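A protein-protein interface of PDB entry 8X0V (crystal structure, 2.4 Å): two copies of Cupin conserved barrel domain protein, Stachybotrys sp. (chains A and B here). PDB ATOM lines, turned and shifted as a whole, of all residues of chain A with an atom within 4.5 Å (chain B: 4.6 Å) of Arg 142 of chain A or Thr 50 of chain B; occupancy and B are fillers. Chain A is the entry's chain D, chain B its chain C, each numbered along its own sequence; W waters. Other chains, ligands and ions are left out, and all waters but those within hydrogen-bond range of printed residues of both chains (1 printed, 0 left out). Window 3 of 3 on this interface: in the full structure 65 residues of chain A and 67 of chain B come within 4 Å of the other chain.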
ATOM      1  N   PHE A 132      12.497 -27.676  19.770  1.00  0.00           N
ATOM      2  CA  PHE A 132      11.213 -27.738  19.091  1.00  0.00           C
ATOM      3  C   PHE A 132      11.398 -27.958  17.597  1.00  0.00           C
ATOM      4  O   PHE A 132      12.405 -27.552  17.007  1.00  0.00           O
ATOM      5  CB  PHE A 132      10.400 -26.464  19.328  1.00  0.00           C
ATOM      6  CG  PHE A 132       9.829 -26.366  20.708  1.00  0.00           C
ATOM      7  CD1 PHE A 132      10.558 -25.782  21.733  1.00  0.00           C
ATOM      8  CD2 PHE A 132       8.569 -26.866  20.987  1.00  0.00           C
ATOM      9  CE1 PHE A 132      10.037 -25.695  23.007  1.00  0.00           C
ATOM     10  CE2 PHE A 132       8.039 -26.782  22.260  1.00  0.00           C
ATOM     11  CZ  PHE A 132       8.773 -26.195  23.272  1.00  0.00           C
ATOM     12  N   LYS A 133      10.408 -28.604  16.993  1.00  0.00           N
ATOM     13  CA  LYS A 133      10.344 -28.798  15.553  1.00  0.00           C
ATOM     14  C   LYS A 133       9.199 -27.961  15.000  1.00  0.00           C
ATOM     15  O   LYS A 133       8.058 -28.079  15.464  1.00  0.00           O
ATOM     16  CB  LYS A 133      10.146 -30.278  15.211  1.00  0.00           C
ATOM     17  CG  LYS A 133      10.212 -30.588  13.728  1.00  0.00           C
ATOM     18  CD  LYS A 133      10.123 -32.087  13.468  1.00  0.00           C
ATOM     19  CE  LYS A 133      11.494 -32.742  13.516  1.00  0.00           C
ATOM     20  NZ  LYS A 133      11.489 -34.094  12.891  1.00  0.00           N
ATOM     21  N   LEU A 134       9.504 -27.111  14.026  1.00  0.00           N
ATOM     22  CA  LEU A 134       8.508 -26.271  13.370  1.00  0.00           C
ATOM     23  C   LEU A 134       8.238 -26.853  11.988  1.00  0.00           C
ATOM     24  O   LEU A 134       9.073 -26.733  11.085  1.00  0.00           O
ATOM     25  CB  LEU A 134       8.983 -24.824  13.274  1.00  0.00           C
ATOM     26  CG  LEU A 134       8.056 -23.884  12.499  1.00  0.00           C
ATOM     27  CD1 LEU A 134       6.761 -23.651  13.267  1.00  0.00           C
ATOM     28  CD2 LEU A 134       8.751 -22.566  12.193  1.00  0.00           C
ATOM     29  N   GLU A 141      10.501 -28.468   7.374  1.00  0.00           N
ATOM     30  CA  GLU A 141      10.615 -28.379   8.819  1.00  0.00           C
ATOM     31  C   GLU A 141      11.970 -27.809   9.206  1.00  0.00           C
ATOM     32  O   GLU A 141      12.960 -27.960   8.486  1.00  0.00           O
ATOM     33  CB  GLU A 141      10.414 -29.743   9.486  1.00  0.00           C
ATOM     34  CG  GLU A 141      11.293 -30.849   8.929  1.00  0.00           C
ATOM     35  CD  GLU A 141      11.220 -32.114   9.758  1.00  0.00           C
ATOM     36  OE1 GLU A 141      12.252 -32.501  10.346  1.00  0.00           O
ATOM     37  OE2 GLU A 141      10.126 -32.717   9.826  1.00  0.00           O
ATOM     38  N   ARG A 142      11.993 -27.150  10.361  1.00  0.00           N
ATOM     39  CA  ARG A 142      13.216 -26.677  10.986  1.00  0.00           C
ATOM     40  C   ARG A 142      13.207 -27.093  12.446  1.00  0.00           C
ATOM     41  O   ARG A 142      12.155 -27.090  13.093  1.00  0.00           O
ATOM     42  CB  ARG A 142      13.358 -25.153  10.888  1.00  0.00           C
ATOM     43  CG  ARG A 142      13.616 -24.632   9.493  1.00  0.00           C
ATOM     44  CD  ARG A 142      14.974 -25.057   8.975  1.00  0.00           C
ATOM     45  NE  ARG A 142      15.204 -24.552   7.625  1.00  0.00           N
ATOM     46  CZ  ARG A 142      14.712 -25.112   6.524  1.00  0.00           C
ATOM     47  NH1 ARG A 142      13.960 -26.199   6.608  1.00  0.00           N
ATOM     48  NH2 ARG A 142      14.972 -24.583   5.337  1.00  0.00           N
ATOM     49  N   ILE A 143      14.375 -27.453  12.960  1.00  0.00           N
ATOM     50  CA  ILE A 143      14.555 -27.745  14.375  1.00  0.00           C
ATOM     51  C   ILE A 143      15.108 -26.495  15.042  1.00  0.00           C
ATOM     52  O   ILE A 143      16.121 -25.940  14.596  1.00  0.00           O
ATOM     53  CB  ILE A 143      15.483 -28.954  14.583  1.00  0.00           C
ATOM     54  CG1 ILE A 143      14.710 -30.253  14.353  1.00  0.00           C
ATOM     55  CG2 ILE A 143      16.092 -28.933  15.982  1.00  0.00           C
ATOM     56  CD1 ILE A 143      15.573 -31.488  14.341  1.00  0.00           C
ATOM     57  N   MET A 144      14.436 -26.038  16.093  1.00  0.00           N
ATOM     58  CA  MET A 144      14.807 -24.813  16.791  1.00  0.00           C
ATOM     59  C   MET A 144      15.246 -25.161  18.203  1.00  0.00           C
ATOM     60  O   MET A 144      14.485 -25.774  18.961  1.00  0.00           O
ATOM     61  CB  MET A 144      13.642 -23.820  16.817  1.00  0.00           C
ATOM     62  CG  MET A 144      13.399 -23.125  15.487  1.00  0.00           C
ATOM     63  SD  MET A 144      11.978 -22.014  15.512  1.00  0.00           S
ATOM     64  CE  MET A 144      12.478 -20.837  16.769  1.00  0.00           C
ATOM     65  N   ASN B  33      20.020 -19.234  14.696  1.00  0.00           N
ATOM     66  CA  ASN B  33      19.271 -19.407  13.462  1.00  0.00           C
ATOM     67  C   ASN B  33      18.033 -18.525  13.531  1.00  0.00           C
ATOM     68  O   ASN B  33      17.267 -18.602  14.498  1.00  0.00           O
ATOM     69  CB  ASN B  33      18.854 -20.867  13.255  1.00  0.00           C
ATOM     70  CG  ASN B  33      19.976 -21.728  12.717  1.00  0.00           C
ATOM     71  OD1 ASN B  33      20.745 -21.305  11.855  1.00  0.00           O
ATOM     72  ND2 ASN B  33      20.066 -22.951  13.216  1.00  0.00           N
ATOM     73  N   ARG B  34      17.848 -17.679  12.525  1.00  0.00           N
ATOM     74  CA  ARG B  34      16.599 -16.954  12.341  1.00  0.00           C
ATOM     75  C   ARG B  34      15.864 -17.577  11.165  1.00  0.00           C
ATOM     76  O   ARG B  34      16.415 -17.665  10.062  1.00  0.00           O
ATOM     77  CB  ARG B  34      16.831 -15.464  12.099  1.00  0.00           C
ATOM     78  CG  ARG B  34      15.550 -14.720  11.763  1.00  0.00           C
ATOM     79  CD  ARG B  34      15.814 -13.301  11.306  1.00  0.00           C
ATOM     80  NE  ARG B  34      16.470 -13.230  10.004  1.00  0.00           N
ATOM     81  CZ  ARG B  34      16.473 -12.147   9.232  1.00  0.00           C
ATOM     82  NH1 ARG B  34      15.849 -11.045   9.628  1.00  0.00           N
ATOM     83  NH2 ARG B  34      17.099 -12.167   8.063  1.00  0.00           N
ATOM     84  N   HIS B  35      14.633 -18.013  11.401  1.00  0.00           N
ATOM     85  CA  HIS B  35      13.805 -18.630  10.376  1.00  0.00           C
ATOM     86  C   HIS B  35      12.654 -17.698  10.029  1.00  0.00           C
ATOM     87  O   HIS B  35      11.930 -17.243  10.920  1.00  0.00           O
ATOM     88  CB  HIS B  35      13.268 -19.985  10.843  1.00  0.00           C
ATOM     89  CG  HIS B  35      14.333 -20.941  11.287  1.00  0.00           C
ATOM     90  ND1 HIS B  35      15.205 -21.545  10.408  1.00  0.00           N
ATOM     91  CD2 HIS B  35      14.656 -21.403  12.517  1.00  0.00           C
ATOM     92  CE1 HIS B  35      16.023 -22.336  11.078  1.00  0.00           C
ATOM     93  NE2 HIS B  35      15.714 -22.266  12.359  1.00  0.00           N
ATOM     94  N   PHE B  47       9.639 -22.245   4.086  1.00  0.00           N
ATOM     95  CA  PHE B  47      10.677 -21.446   4.719  1.00  0.00           C
ATOM     96  C   PHE B  47      11.374 -20.612   3.656  1.00  0.00           C
ATOM     97  O   PHE B  47      11.837 -21.147   2.642  1.00  0.00           O
ATOM     98  CB  PHE B  47      11.689 -22.332   5.450  1.00  0.00           C
ATOM     99  CG  PHE B  47      11.194 -22.850   6.767  1.00  0.00           C
ATOM    100  CD1 PHE B  47      11.253 -22.057   7.902  1.00  0.00           C
ATOM    101  CD2 PHE B  47      10.655 -24.124   6.868  1.00  0.00           C
ATOM    102  CE1 PHE B  47      10.789 -22.527   9.114  1.00  0.00           C
ATOM    103  CE2 PHE B  47      10.191 -24.600   8.079  1.00  0.00           C
ATOM    104  CZ  PHE B  47      10.257 -23.802   9.202  1.00  0.00           C
ATOM    105  N   SER B  49      13.985 -18.327   4.461  1.00  0.00           N
ATOM    106  CA  SER B  49      15.384 -18.087   4.783  1.00  0.00           C
ATOM    107  C   SER B  49      15.722 -18.664   6.149  1.00  0.00           C
ATOM    108  O   SER B  49      14.862 -18.783   7.026  1.00  0.00           O
ATOM    109  CB  SER B  49      15.713 -16.589   4.755  1.00  0.00           C
ATOM    110  OG  SER B  49      14.881 -15.876   5.652  1.00  0.00           O
ATOM    111  N   THR B  50      16.996 -19.025   6.301  1.00  0.00           N
ATOM    112  CA  THR B  50      17.608 -19.359   7.582  1.00  0.00           C
ATOM    113  C   THR B  50      18.943 -18.631   7.636  1.00  0.00           C
ATOM    114  O   THR B  50      19.800 -18.852   6.774  1.00  0.00           O
ATOM    115  CB  THR B  50      17.813 -20.870   7.732  1.00  0.00           C
ATOM    116  OG1 THR B  50      16.545 -21.538   7.692  1.00  0.00           O
ATOM    117  CG2 THR B  50      18.513 -21.185   9.046  1.00  0.00           C
ATOM    118  N   ASP B  51      19.125 -17.758   8.622  1.00  0.00           N
ATOM    119  CA  ASP B  51      20.309 -16.905   8.627  1.00  0.00           C
ATOM    120  C   ASP B  51      20.626 -16.464  10.049  1.00  0.00           C
ATOM    121  O   ASP B  51      19.976 -16.873  11.014  1.00  0.00           O
ATOM    122  CB  ASP B  51      20.115 -15.699   7.701  1.00  0.00           C
ATOM    123  CG  ASP B  51      18.822 -14.953   7.975  1.00  0.00           C
ATOM    124  OD1 ASP B  51      18.540 -14.643   9.155  1.00  0.00           O
ATOM    125  OD2 ASP B  51      18.083 -14.670   7.005  1.00  0.00           O
HETATM  126  O   HOH W   1      17.255 -23.652  14.426  1.00  0.00           O
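OG1 of Thr 50 of chain B lies within hydrogen-bond range of NE of Arg 142 of chain A, 3.3 Å away.
A ring nitrogen (ND1) of His 35 of chain B lies within hydrogen-bond range of the side-chain hydroxyl (OG1) of Thr 50 of chain B (3.0 Å). The backbone carbonyl oxygen of Phe 132 of chain A lies within hydrogen-bond range of the backbone NH of Met 144 of chain A, 2.7 Å away. NZ of Lys 133 of chain A lies within salt-bridge range of OE1 of Glu 141 of chain A (3.1 Å). The backbone NH (N) of Leu 134 of chain A lies within hydrogen-bond range of the backbone carbonyl oxygen (O) of Arg 142 of chain A, 2.8 Å away.
Among the printed residues, pairs that only touch across the chains: Leu 134 of chain A with Phe 47 of chain B (3.6 Å), Glu 141 of chain A with Phe 47 of chain B (3.8 Å), Arg 142 of chain A with His 35 of chain B (3.6 Å), Arg 142 of chain A with Phe 47 of chain B (3.5 Å) and Met 144 of chain A with His 35 of chain B (3.7 Å).
Printed residues of chain A within 4 Å of Thr 50 of chain B: Arg 142. Of the printed residues of chain B, Glu 141 of chain A touches Phe 47. Of the printed residues of chain A, His 35 of chain B touches Arg 142 (3.6 Å) and Met 144 (3.7 Å). Of the printed residues of chain B, Met 144 of chain A touches His 35 (3.7 Å). Of the printed residues of chain A, Phe 47 of chain B touches Leu 134, Glu 141 and Arg 142. Of the printed residues of chain B, Leu 134 of chain A touches Phe 47. Ile 143 of chain A touches none of the printed residues of chain B. Ser 49 of chain B touches none of the printed residues of chain A. The nearest printed residue of chain B that does not touch Arg 142 of chain A is Ser 49 of chain B (5.8 Å). The nearest printed residue of chain A that does not touch Thr 50 of chain B is Glu 141 of chain A (7.4 Å). The nearest printed residue of chain B that does not touch Glu 141 of chain A is His 35 of chain B (6.9 Å).
Along chain B the printed residues that touch a printed residue of chain A span positions 35 to 50. Of the 7 printed residues of chain A, 4 touch a printed residue of chain B. Hydrophobic or aromatic side chains of chain A within 4 Å of the printed part of chain B: Leu 134 and Met 144. Among the printed residues, 6 pairs touch across the chains. Among the printed residues, no Asp or Glu carboxylate lies within 4 Å of a Lys or Arg side-chain nitrogen of the other chain.
No position is printed for both chains. Of the 6 pairs that touch across the chains among the printed residues, none has its exchanged pair printed and touching as well.
Water W1 lies within hydrogen-bond range of O of Ile 143 of chain A, NE2 of His 35 of chain B and ND2 of Asn 33 of chain B.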
